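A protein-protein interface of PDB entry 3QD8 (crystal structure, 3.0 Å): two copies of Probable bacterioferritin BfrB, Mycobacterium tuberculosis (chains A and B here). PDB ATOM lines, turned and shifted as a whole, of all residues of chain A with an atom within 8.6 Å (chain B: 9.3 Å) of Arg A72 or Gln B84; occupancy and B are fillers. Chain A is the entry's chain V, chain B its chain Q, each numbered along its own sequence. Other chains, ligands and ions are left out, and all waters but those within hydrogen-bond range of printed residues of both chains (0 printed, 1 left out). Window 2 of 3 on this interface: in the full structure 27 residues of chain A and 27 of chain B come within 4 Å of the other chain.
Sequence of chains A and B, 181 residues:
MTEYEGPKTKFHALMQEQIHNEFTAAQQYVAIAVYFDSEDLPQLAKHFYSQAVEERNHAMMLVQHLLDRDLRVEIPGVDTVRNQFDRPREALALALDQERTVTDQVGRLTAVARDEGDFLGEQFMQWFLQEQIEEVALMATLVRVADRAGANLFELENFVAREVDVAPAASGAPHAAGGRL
O of Arg A72 sits at hydrogen-bond distance from NE2 of His A12 (2.8 Å). The side-chain hydroxyl (OG) of Ser B38 is in hydrogen-bond range of the backbone carbonyl oxygen (O) of Tyr B35 (2.7 Å). O of Glu A74 lies within hydrogen-bond range of NE2 of Gln A16.
Hydrophobic or aromatic side chains of chain B within 4 Å of the printed part of chain A: Ala B31, Val B34 and Val B81. Printed residues of chain A that touch a printed residue of chain B: Val A63, Leu A67, Arg A72, Val A73, Glu A74 and Ile A75.
Among the printed residues, pairs that only touch across the chains: Val A63 with Val B34, Leu A67 with Ser B38, Arg A72 with Gln B84, Val A73 with Val B34, Glu A74 with Asn B83, Ile A75 with Ala B31, Ile A75 with Val B34 and Ile A75 with Val B81.
The backbone carbonyl oxygen (O) of Ile A75 sits at hydrogen-bond distance from the side-chain amide nitrogen (ND2) of Asn B83.
Printed residues of chain B within 4 Å of Val A63: Val B34. His A65 touches none of the printed residues of chain B. Of chain B, only Gln B84 comes within 4 Å of Arg A72. Val A73 touches one residue of chain B. Printed residues of chain B within 4 Å of Ile A75: Ala B31 (3.5 Å), Val B34 (3.7 Å), Val B81 (3.7 Å) and Asn B83 (2.8 Å). Tyr B35 touches none of the printed residues of chain A. Of the printed residues of chain A, Ser B38 touches Leu A67 (3.6 Å). Gln B84 touches just one residue of chain A: Arg A72. Phe B85 touches none of the printed residues of chain A. The nearest residue of chain A that does not touch Gln B84 is Glu A74 (4.6 Å). The nearest printed residue of chain B that does not touch Leu A67 is Val B34 (4.3 Å).
No position is printed for both chains.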
ATOM      1  N   HIS A  12      -7.023 -27.675  -1.322  1.00  0.00           N
ATOM      2  CA  HIS A  12      -6.673 -26.319  -0.976  1.00  0.00           C
ATOM      3  C   HIS A  12      -6.512 -25.492  -2.240  1.00  0.00           C
ATOM      4  O   HIS A  12      -7.013 -24.370  -2.318  1.00  0.00           O
ATOM      5  CB  HIS A  12      -5.379 -26.341  -0.171  1.00  0.00           C
ATOM      6  CG  HIS A  12      -4.856 -24.985   0.183  1.00  0.00           C
ATOM      7  ND1 HIS A  12      -3.522 -24.748   0.423  1.00  0.00           N
ATOM      8  CD2 HIS A  12      -5.485 -23.797   0.348  1.00  0.00           C
ATOM      9  CE1 HIS A  12      -3.350 -23.470   0.711  1.00  0.00           C
ATOM     10  NE2 HIS A  12      -4.524 -22.870   0.672  1.00  0.00           N
ATOM     11  N   ALA A  13      -5.835 -26.055  -3.237  1.00  0.00           N
ATOM     12  CA  ALA A  13      -5.612 -25.345  -4.500  1.00  0.00           C
ATOM     13  C   ALA A  13      -6.919 -25.096  -5.239  1.00  0.00           C
ATOM     14  O   ALA A  13      -7.126 -24.031  -5.825  1.00  0.00           O
ATOM     15  CB  ALA A  13      -4.677 -26.114  -5.372  1.00  0.00           C
ATOM     16  N   MET A  15      -9.859 -24.897  -3.855  1.00  0.00           N
ATOM     17  CA  MET A  15     -10.621 -23.957  -3.048  1.00  0.00           C
ATOM     18  C   MET A  15     -10.223 -22.521  -3.377  1.00  0.00           C
ATOM     19  O   MET A  15     -11.069 -21.624  -3.480  1.00  0.00           O
ATOM     20  CB  MET A  15     -10.377 -24.264  -1.562  1.00  0.00           C
ATOM     21  CG  MET A  15     -10.840 -23.198  -0.548  1.00  0.00           C
ATOM     22  SD  MET A  15     -12.547 -23.393   0.014  1.00  0.00           S
ATOM     23  CE  MET A  15     -12.678 -25.165   0.002  1.00  0.00           C
ATOM     24  N   GLN A  16      -8.922 -22.302  -3.538  1.00  0.00           N
ATOM     25  CA  GLN A  16      -8.430 -20.993  -3.947  1.00  0.00           C
ATOM     26  C   GLN A  16      -9.063 -20.584  -5.264  1.00  0.00           C
ATOM     27  O   GLN A  16      -9.543 -19.469  -5.431  1.00  0.00           O
ATOM     28  CB  GLN A  16      -6.917 -21.014  -4.117  1.00  0.00           C
ATOM     29  CG  GLN A  16      -6.360 -19.704  -4.650  1.00  0.00           C
ATOM     30  CD  GLN A  16      -6.604 -18.540  -3.710  1.00  0.00           C
ATOM     31  OE1 GLN A  16      -6.248 -18.593  -2.528  1.00  0.00           O
ATOM     32  NE2 GLN A  16      -7.217 -17.479  -4.232  1.00  0.00           N
ATOM     33  N   ILE A  19     -12.564 -19.384  -4.902  1.00  0.00           N
ATOM     34  CA  ILE A  19     -12.596 -17.986  -4.489  1.00  0.00           C
ATOM     35  C   ILE A  19     -12.572 -17.050  -5.693  1.00  0.00           C
ATOM     36  O   ILE A  19     -13.337 -16.095  -5.762  1.00  0.00           O
ATOM     37  CB  ILE A  19     -11.402 -17.646  -3.588  1.00  0.00           C
ATOM     38  CG1 ILE A  19     -11.543 -18.360  -2.253  1.00  0.00           C
ATOM     39  CG2 ILE A  19     -11.306 -16.147  -3.385  1.00  0.00           C
ATOM     40  CD1 ILE A  19     -10.426 -18.092  -1.331  1.00  0.00           C
ATOM     41  N   LEU A  62     -15.375 -18.596   1.730  1.00  0.00           N
ATOM     42  CA  LEU A  62     -14.277 -19.458   1.358  1.00  0.00           C
ATOM     43  C   LEU A  62     -12.993 -18.853   1.905  1.00  0.00           C
ATOM     44  O   LEU A  62     -12.185 -19.562   2.504  1.00  0.00           O
ATOM     45  CB  LEU A  62     -14.219 -19.640  -0.163  1.00  0.00           C
ATOM     46  CG  LEU A  62     -15.507 -20.244  -0.735  1.00  0.00           C
ATOM     47  CD1 LEU A  62     -15.449 -20.344  -2.235  1.00  0.00           C
ATOM     48  CD2 LEU A  62     -15.764 -21.613  -0.132  1.00  0.00           C
ATOM     49  N   VAL A  63     -12.804 -17.546   1.720  1.00  0.00           N
ATOM     50  CA  VAL A  63     -11.634 -16.870   2.293  1.00  0.00           C
ATOM     51  C   VAL A  63     -11.540 -17.217   3.773  1.00  0.00           C
ATOM     52  O   VAL A  63     -10.488 -17.587   4.276  1.00  0.00           O
ATOM     53  CB  VAL A  63     -11.716 -15.339   2.176  1.00  0.00           C
ATOM     54  CG1 VAL A  63     -10.456 -14.713   2.735  1.00  0.00           C
ATOM     55  CG2 VAL A  63     -11.927 -14.919   0.747  1.00  0.00           C
ATOM     56  N   HIS A  65     -12.729 -19.736   5.453  1.00  0.00           N
ATOM     57  CA  HIS A  65     -12.430 -21.129   5.736  1.00  0.00           C
ATOM     58  C   HIS A  65     -10.934 -21.370   5.720  1.00  0.00           C
ATOM     59  O   HIS A  65     -10.407 -22.011   6.619  1.00  0.00           O
ATOM     60  CB  HIS A  65     -13.133 -22.067   4.754  1.00  0.00           C
ATOM     61  CG  HIS A  65     -12.772 -23.513   4.936  1.00  0.00           C
ATOM     62  ND1 HIS A  65     -13.368 -24.312   5.891  1.00  0.00           N
ATOM     63  CD2 HIS A  65     -11.879 -24.303   4.289  1.00  0.00           C
ATOM     64  CE1 HIS A  65     -12.852 -25.528   5.830  1.00  0.00           C
ATOM     65  NE2 HIS A  65     -11.944 -25.547   4.870  1.00  0.00           N
ATOM     66  N   LEU A  66     -10.255 -20.853   4.702  1.00  0.00           N
ATOM     67  CA  LEU A  66      -8.802 -20.981   4.620  1.00  0.00           C
ATOM     68  C   LEU A  66      -8.122 -20.255   5.780  1.00  0.00           C
ATOM     69  O   LEU A  66      -7.194 -20.794   6.401  1.00  0.00           O
ATOM     70  CB  LEU A  66      -8.277 -20.473   3.268  1.00  0.00           C
ATOM     71  CG  LEU A  66      -8.751 -21.247   2.034  1.00  0.00           C
ATOM     72  CD1 LEU A  66      -8.101 -20.688   0.793  1.00  0.00           C
ATOM     73  CD2 LEU A  66      -8.402 -22.712   2.198  1.00  0.00           C
ATOM     74  N   LEU A  67      -8.599 -19.042   6.069  1.00  0.00           N
ATOM     75  CA  LEU A  67      -8.145 -18.283   7.230  1.00  0.00           C
ATOM     76  C   LEU A  67      -8.217 -19.132   8.501  1.00  0.00           C
ATOM     77  O   LEU A  67      -7.212 -19.251   9.224  1.00  0.00           O
ATOM     78  CB  LEU A  67      -8.979 -17.021   7.415  1.00  0.00           C
ATOM     79  CG  LEU A  67      -8.633 -15.818   6.554  1.00  0.00           C
ATOM     80  CD1 LEU A  67      -9.546 -14.631   6.891  1.00  0.00           C
ATOM     81  CD2 LEU A  67      -7.170 -15.466   6.735  1.00  0.00           C
ATOM     82  N   ARG A  69      -8.261 -22.237   8.862  1.00  0.00           N
ATOM     83  CA  ARG A  69      -7.402 -23.408   8.825  1.00  0.00           C
ATOM     84  C   ARG A  69      -5.962 -23.033   8.633  1.00  0.00           C
ATOM     85  O   ARG A  69      -5.124 -23.902   8.385  1.00  0.00           O
ATOM     86  CB  ARG A  69      -7.837 -24.376   7.742  1.00  0.00           C
ATOM     87  CG  ARG A  69      -9.133 -25.059   8.074  1.00  0.00           C
ATOM     88  CD  ARG A  69      -9.596 -25.939   6.955  1.00  0.00           C
ATOM     89  NE  ARG A  69      -8.791 -27.150   6.861  1.00  0.00           N
ATOM     90  CZ  ARG A  69      -8.953 -28.068   5.908  1.00  0.00           C
ATOM     91  NH1 ARG A  69      -9.891 -27.897   4.975  1.00  0.00           N
ATOM     92  NH2 ARG A  69      -8.179 -29.151   5.885  1.00  0.00           N
ATOM     93  N   ASP A  70      -5.670 -21.742   8.774  1.00  0.00           N
ATOM     94  CA  ASP A  70      -4.300 -21.252   8.626  1.00  0.00           C
ATOM     95  C   ASP A  70      -3.664 -21.842   7.360  1.00  0.00           C
ATOM     96  O   ASP A  70      -2.544 -22.348   7.385  1.00  0.00           O
ATOM     97  CB  ASP A  70      -3.461 -21.566   9.875  1.00  0.00           C
ATOM     98  CG  ASP A  70      -4.173 -21.154  11.173  1.00  0.00           C
ATOM     99  OD1 ASP A  70      -4.275 -19.933  11.447  1.00  0.00           O
ATOM    100  OD2 ASP A  70      -4.652 -22.048  11.914  1.00  0.00           O
ATOM    101  N   LEU A  71      -4.419 -21.798   6.265  1.00  0.00           N
ATOM    102  CA  LEU A  71      -3.912 -22.121   4.947  1.00  0.00           C
ATOM    103  C   LEU A  71      -3.758 -20.838   4.145  1.00  0.00           C
ATOM    104  O   LEU A  71      -4.481 -19.867   4.376  1.00  0.00           O
ATOM    105  CB  LEU A  71      -4.886 -23.047   4.236  1.00  0.00           C
ATOM    106  CG  LEU A  71      -5.010 -24.420   4.894  1.00  0.00           C
ATOM    107  CD1 LEU A  71      -6.091 -25.262   4.217  1.00  0.00           C
ATOM    108  CD2 LEU A  71      -3.651 -25.108   4.849  1.00  0.00           C
ATOM    109  N   ARG A  72      -2.814 -20.834   3.204  1.00  0.00           N
ATOM    110  CA  ARG A  72      -2.525 -19.646   2.406  1.00  0.00           C
ATOM    111  C   ARG A  72      -3.743 -19.236   1.594  1.00  0.00           C
ATOM    112  O   ARG A  72      -4.338 -20.066   0.901  1.00  0.00           O
ATOM    113  CB  ARG A  72      -1.351 -19.918   1.469  1.00  0.00           C
ATOM    114  CG  ARG A  72      -1.103 -18.831   0.449  1.00  0.00           C
ATOM    115  CD  ARG A  72      -0.279 -17.726   1.050  1.00  0.00           C
ATOM    116  NE  ARG A  72       0.925 -18.286   1.637  1.00  0.00           N
ATOM    117  CZ  ARG A  72       1.597 -17.726   2.637  1.00  0.00           C
ATOM    118  NH1 ARG A  72       1.181 -16.577   3.155  1.00  0.00           N
ATOM    119  NH2 ARG A  72       2.685 -18.316   3.119  1.00  0.00           N
ATOM    120  N   VAL A  73      -4.122 -17.965   1.677  1.00  0.00           N
ATOM    121  CA  VAL A  73      -5.242 -17.483   0.865  1.00  0.00           C
ATOM    122  C   VAL A  73      -4.912 -16.200   0.114  1.00  0.00           C
ATOM    123  O   VAL A  73      -4.148 -15.365   0.594  1.00  0.00           O
ATOM    124  CB  VAL A  73      -6.512 -17.239   1.695  1.00  0.00           C
ATOM    125  CG1 VAL A  73      -6.308 -16.056   2.649  1.00  0.00           C
ATOM    126  CG2 VAL A  73      -7.687 -16.999   0.769  1.00  0.00           C
ATOM    127  N   GLU A  74      -5.497 -16.046  -1.067  1.00  0.00           N
ATOM    128  CA  GLU A  74      -5.204 -14.889  -1.905  1.00  0.00           C
ATOM    129  C   GLU A  74      -6.454 -14.301  -2.521  1.00  0.00           C
ATOM    130  O   GLU A  74      -7.332 -15.027  -2.998  1.00  0.00           O
ATOM    131  CB  GLU A  74      -4.187 -15.249  -2.989  1.00  0.00           C
ATOM    132  CG  GLU A  74      -2.787 -14.876  -2.586  1.00  0.00           C
ATOM    133  CD  GLU A  74      -1.761 -15.748  -3.227  1.00  0.00           C
ATOM    134  OE1 GLU A  74      -2.169 -16.669  -3.952  1.00  0.00           O
ATOM    135  OE2 GLU A  74      -0.555 -15.515  -2.999  1.00  0.00           O
ATOM    136  N   ILE A  75      -6.531 -12.976  -2.486  1.00  0.00           N
ATOM    137  CA  ILE A  75      -7.620 -12.263  -3.124  1.00  0.00           C
ATOM    138  C   ILE A  75      -7.231 -12.063  -4.578  1.00  0.00           C
ATOM    139  O   ILE A  75      -6.290 -11.330  -4.877  1.00  0.00           O
ATOM    140  CB  ILE A  75      -7.891 -10.908  -2.455  1.00  0.00           C
ATOM    141  CG1 ILE A  75      -8.204 -11.105  -0.975  1.00  0.00           C
ATOM    142  CG2 ILE A  75      -9.063 -10.205  -3.109  1.00  0.00           C
ATOM    143  CD1 ILE A  75      -9.398 -11.981  -0.722  1.00  0.00           C
ATOM    144  N   GLN B  28      -8.184  -4.477  -3.963  1.00  0.00           N
ATOM    145  CA  GLN B  28      -6.895  -4.378  -3.280  1.00  0.00           C
ATOM    146  C   GLN B  28      -7.081  -4.163  -1.768  1.00  0.00           C
ATOM    147  O   GLN B  28      -6.283  -4.633  -0.939  1.00  0.00           O
ATOM    148  CB  GLN B  28      -6.063  -3.248  -3.878  1.00  0.00           C
ATOM    149  CG  GLN B  28      -4.781  -2.985  -3.136  1.00  0.00           C
ATOM    150  CD  GLN B  28      -3.821  -4.167  -3.177  1.00  0.00           C
ATOM    151  OE1 GLN B  28      -3.151  -4.424  -4.189  1.00  0.00           O
ATOM    152  NE2 GLN B  28      -3.734  -4.879  -2.061  1.00  0.00           N
ATOM    153  N   ALA B  31      -7.868  -7.426  -0.227  1.00  0.00           N
ATOM    154  CA  ALA B  31      -6.601  -8.135  -0.099  1.00  0.00           C
ATOM    155  C   ALA B  31      -5.865  -7.700   1.160  1.00  0.00           C
ATOM    156  O   ALA B  31      -5.428  -8.531   1.953  1.00  0.00           O
ATOM    157  CB  ALA B  31      -5.746  -7.905  -1.333  1.00  0.00           C
ATOM    158  N   ILE B  32      -5.739  -6.388   1.328  1.00  0.00           N
ATOM    159  CA  ILE B  32      -5.166  -5.813   2.535  1.00  0.00           C
ATOM    160  C   ILE B  32      -5.927  -6.200   3.799  1.00  0.00           C
ATOM    161  O   ILE B  32      -5.314  -6.512   4.815  1.00  0.00           O
ATOM    162  CB  ILE B  32      -5.110  -4.287   2.436  1.00  0.00           C
ATOM    163  CG1 ILE B  32      -4.161  -3.881   1.297  1.00  0.00           C
ATOM    164  CG2 ILE B  32      -4.704  -3.679   3.797  1.00  0.00           C
ATOM    165  CD1 ILE B  32      -4.114  -2.390   0.995  1.00  0.00           C
ATOM    166  N   VAL B  34      -7.856  -8.897   4.275  1.00  0.00           N
ATOM    167  CA  VAL B  34      -7.591 -10.312   4.497  1.00  0.00           C
ATOM    168  C   VAL B  34      -6.172 -10.552   5.042  1.00  0.00           C
ATOM    169  O   VAL B  34      -5.960 -11.436   5.869  1.00  0.00           O
ATOM    170  CB  VAL B  34      -7.832 -11.152   3.210  1.00  0.00           C
ATOM    171  CG1 VAL B  34      -7.270 -12.537   3.369  1.00  0.00           C
ATOM    172  CG2 VAL B  34      -9.310 -11.239   2.895  1.00  0.00           C
ATOM    173  N   TYR B  35      -5.203  -9.769   4.578  1.00  0.00           N
ATOM    174  CA  TYR B  35      -3.842  -9.865   5.100  1.00  0.00           C
ATOM    175  C   TYR B  35      -3.837  -9.612   6.613  1.00  0.00           C
ATOM    176  O   TYR B  35      -3.385 -10.442   7.389  1.00  0.00           O
ATOM    177  CB  TYR B  35      -2.885  -8.899   4.367  1.00  0.00           C
ATOM    178  CG  TYR B  35      -1.583  -8.664   5.106  1.00  0.00           C
ATOM    179  CD1 TYR B  35      -0.586  -9.620   5.118  1.00  0.00           C
ATOM    180  CD2 TYR B  35      -1.370  -7.490   5.817  1.00  0.00           C
ATOM    181  CE1 TYR B  35       0.588  -9.424   5.814  1.00  0.00           C
ATOM    182  CE2 TYR B  35      -0.190  -7.269   6.517  1.00  0.00           C
ATOM    183  CZ  TYR B  35       0.790  -8.239   6.516  1.00  0.00           C
ATOM    184  OH  TYR B  35       1.968  -8.018   7.214  1.00  0.00           O
ATOM    185  N   SER B  38      -5.376 -12.315   8.687  1.00  0.00           N
ATOM    186  CA  SER B  38      -4.496 -13.476   8.879  1.00  0.00           C
ATOM    187  C   SER B  38      -3.345 -13.202   9.830  1.00  0.00           C
ATOM    188  O   SER B  38      -2.780 -14.127  10.399  1.00  0.00           O
ATOM    189  CB  SER B  38      -3.941 -13.991   7.550  1.00  0.00           C
ATOM    190  OG  SER B  38      -3.032 -13.077   6.960  1.00  0.00           O
ATOM    191  N   GLU B  39      -2.995 -11.933   9.989  1.00  0.00           N
ATOM    192  CA  GLU B  39      -1.959 -11.554  10.927  1.00  0.00           C
ATOM    193  C   GLU B  39      -2.552 -11.323  12.316  1.00  0.00           C
ATOM    194  O   GLU B  39      -1.873 -10.803  13.204  1.00  0.00           O
ATOM    195  CB  GLU B  39      -1.273 -10.286  10.447  1.00  0.00           C
ATOM    196  CG  GLU B  39      -0.470 -10.446   9.185  1.00  0.00           C
ATOM    197  CD  GLU B  39       0.796 -11.218   9.419  1.00  0.00           C
ATOM    198  OE1 GLU B  39       1.320 -11.176  10.552  1.00  0.00           O
ATOM    199  OE2 GLU B  39       1.284 -11.873   8.474  1.00  0.00           O
ATOM    200  N   VAL B  81      -4.370  -8.090  -7.625  1.00  0.00           N
ATOM    201  CA  VAL B  81      -3.978  -7.108  -6.625  1.00  0.00           C
ATOM    202  C   VAL B  81      -2.936  -7.748  -5.733  1.00  0.00           C
ATOM    203  O   VAL B  81      -2.781  -8.972  -5.747  1.00  0.00           O
ATOM    204  CB  VAL B  81      -5.173  -6.587  -5.778  1.00  0.00           C
ATOM    205  CG1 VAL B  81      -6.208  -5.936  -6.654  1.00  0.00           C
ATOM    206  CG2 VAL B  81      -5.808  -7.708  -4.958  1.00  0.00           C
ATOM    207  N   ARG B  82      -2.229  -6.932  -4.961  1.00  0.00           N
ATOM    208  CA  ARG B  82      -1.134  -7.438  -4.156  1.00  0.00           C
ATOM    209  C   ARG B  82      -1.623  -8.152  -2.906  1.00  0.00           C
ATOM    210  O   ARG B  82      -2.468  -7.632  -2.192  1.00  0.00           O
ATOM    211  CB  ARG B  82      -0.214  -6.299  -3.751  1.00  0.00           C
ATOM    212  CG  ARG B  82       1.142  -6.775  -3.254  1.00  0.00           C
ATOM    213  CD  ARG B  82       1.821  -5.694  -2.455  1.00  0.00           C
ATOM    214  NE  ARG B  82       3.266  -5.695  -2.639  1.00  0.00           N
ATOM    215  CZ  ARG B  82       4.001  -4.590  -2.605  1.00  0.00           C
ATOM    216  NH1 ARG B  82       3.408  -3.418  -2.398  1.00  0.00           N
ATOM    217  NH2 ARG B  82       5.317  -4.654  -2.781  1.00  0.00           N
ATOM    218  N   ASN B  83      -1.064  -9.326  -2.627  1.00  0.00           N
ATOM    219  CA  ASN B  83      -1.499 -10.125  -1.490  1.00  0.00           C
ATOM    220  C   ASN B  83      -0.451 -10.354  -0.408  1.00  0.00           C
ATOM    221  O   ASN B  83      -0.785 -10.698   0.724  1.00  0.00           O
ATOM    222  CB  ASN B  83      -2.033 -11.476  -1.964  1.00  0.00           C
ATOM    223  CG  ASN B  83      -3.538 -11.480  -2.166  1.00  0.00           C
ATOM    224  OD1 ASN B  83      -4.322 -11.437  -1.197  1.00  0.00           O
ATOM    225  ND2 ASN B  83      -3.952 -11.549  -3.429  1.00  0.00           N
ATOM    226  N   GLN B  84       0.816 -10.175  -0.740  1.00  0.00           N
ATOM    227  CA  GLN B  84       1.859 -10.429   0.246  1.00  0.00           C
ATOM    228  C   GLN B  84       2.568  -9.154   0.670  1.00  0.00           C
ATOM    229  O   GLN B  84       2.906  -8.321  -0.175  1.00  0.00           O
ATOM    230  CB  GLN B  84       2.856 -11.467  -0.274  1.00  0.00           C
ATOM    231  CG  GLN B  84       2.247 -12.868  -0.414  1.00  0.00           C
ATOM    232  CD  GLN B  84       3.299 -13.969  -0.481  1.00  0.00           C
ATOM    233  OE1 GLN B  84       4.435 -13.738  -0.912  1.00  0.00           O
ATOM    234  NE2 GLN B  84       2.922 -15.176  -0.054  1.00  0.00           N
ATOM    235  N   PHE B  85       2.775  -9.008   1.981  1.00  0.00           N
ATOM    236  CA  PHE B  85       3.400  -7.818   2.545  1.00  0.00           C
ATOM    237  C   PHE B  85       4.415  -8.208   3.593  1.00  0.00           C
ATOM    238  O   PHE B  85       4.178  -9.144   4.356  1.00  0.00           O
ATOM    239  CB  PHE B  85       2.347  -6.922   3.190  1.00  0.00           C
ATOM    240  CG  PHE B  85       1.264  -6.494   2.255  1.00  0.00           C
ATOM    241  CD1 PHE B  85       1.408  -5.352   1.494  1.00  0.00           C
ATOM    242  CD2 PHE B  85       0.113  -7.234   2.128  1.00  0.00           C
ATOM    243  CE1 PHE B  85       0.424  -4.954   0.618  1.00  0.00           C
ATOM    244  CE2 PHE B  85      -0.872  -6.841   1.265  1.00  0.00           C
ATOM    245  CZ  PHE B  85      -0.718  -5.697   0.508  1.00  0.00           C
ATOM    246  N   ASP B  86       5.539  -7.494   3.634  1.00  0.00           N
ATOM    247  CA  ASP B  86       6.570  -7.735   4.648  1.00  0.00           C
ATOM    248  C   ASP B  86       6.032  -7.529   6.065  1.00  0.00           C
ATOM    249  O   ASP B  86       6.403  -8.251   6.986  1.00  0.00           O
ATOM    250  CB  ASP B  86       7.775  -6.818   4.429  1.00  0.00           C
ATOM    251  CG  ASP B  86       8.473  -7.082   3.116  1.00  0.00           C
ATOM    252  OD1 ASP B  86       8.825  -8.257   2.852  1.00  0.00           O
ATOM    253  OD2 ASP B  86       8.676  -6.108   2.356  1.00  0.00           O
ATOM    254  N   ARG B  87       5.153  -6.542   6.231  1.00  0.00           N
ATOM    255  CA  ARG B  87       4.618  -6.217   7.547  1.00  0.00           C
ATOM    256  C   ARG B  87       3.495  -5.193   7.438  1.00  0.00           C
ATOM    257  O   ARG B  87       3.410  -4.453   6.452  1.00  0.00           O
ATOM    258  CB  ARG B  87       5.734  -5.657   8.411  1.00  0.00           C
ATOM    259  CG  ARG B  87       6.289  -4.395   7.833  1.00  0.00           C
ATOM    260  CD  ARG B  87       7.326  -3.803   8.719  1.00  0.00           C
ATOM    261  NE  ARG B  87       7.960  -2.676   8.050  1.00  0.00           N
ATOM    262  CZ  ARG B  87       8.523  -1.651   8.682  1.00  0.00           C
ATOM    263  NH1 ARG B  87       8.525  -1.602  10.016  1.00  0.00           N
ATOM    264  NH2 ARG B  87       9.076  -0.670   7.977  1.00  0.00           N
ATOM    265  N   PRO B  88       2.639  -5.139   8.459  1.00  0.00           N
ATOM    266  CA  PRO B  88       1.465  -4.267   8.466  1.00  0.00           C
ATOM    267  C   PRO B  88       1.739  -2.871   7.929  1.00  0.00           C
ATOM    268  O   PRO B  88       0.967  -2.381   7.100  1.00  0.00           O
ATOM    269  CB  PRO B  88       1.126  -4.180   9.947  1.00  0.00           C
ATOM    270  CG  PRO B  88       1.541  -5.510  10.473  1.00  0.00           C
ATOM    271  CD  PRO B  88       2.777  -5.887   9.714  1.00  0.00           C
ATOM    272  N   GLU B  90       3.857  -1.808   5.741  1.00  0.00           N
ATOM    273  CA  GLU B  90       4.001  -1.791   4.284  1.00  0.00           C
ATOM    274  C   GLU B  90       2.655  -1.879   3.549  1.00  0.00           C
ATOM    275  O   GLU B  90       2.479  -1.269   2.498  1.00  0.00           O
ATOM    276  CB  GLU B  90       4.958  -2.874   3.806  1.00  0.00           C
ATOM    277  CG  GLU B  90       5.165  -2.849   2.300  1.00  0.00           C
ATOM    278  CD  GLU B  90       5.910  -4.079   1.781  1.00  0.00           C
ATOM    279  OE1 GLU B  90       6.290  -4.945   2.606  1.00  0.00           O
ATOM    280  OE2 GLU B  90       6.116  -4.176   0.546  1.00  0.00           O
ATOM    281  N   ALA B  91       1.710  -2.622   4.117  1.00  0.00           N
ATOM    282  CA  ALA B  91       0.333  -2.643   3.611  1.00  0.00           C
ATOM    283  C   ALA B  91      -0.367  -1.297   3.758  1.00  0.00           C
ATOM    284  O   ALA B  91      -0.946  -0.798   2.798  1.00  0.00           O
ATOM    285  CB  ALA B  91      -0.483  -3.715   4.301  1.00  0.00           C
ATOM    286  N   LEU B  94       0.858   0.964   0.972  1.00  0.00           N
ATOM    287  CA  LEU B  94       0.234   0.734  -0.313  1.00  0.00           C
ATOM    288  C   LEU B  94      -1.144   1.395  -0.365  1.00  0.00           C
ATOM    289  O   LEU B  94      -1.555   1.940  -1.388  1.00  0.00           O
ATOM    290  CB  LEU B  94       0.114  -0.766  -0.575  1.00  0.00           C
ATOM    291  CG  LEU B  94      -0.596  -1.114  -1.882  1.00  0.00           C
ATOM    292  CD1 LEU B  94       0.209  -0.544  -3.028  1.00  0.00           C
ATOM    293  CD2 LEU B  94      -0.726  -2.614  -2.003  1.00  0.00           C
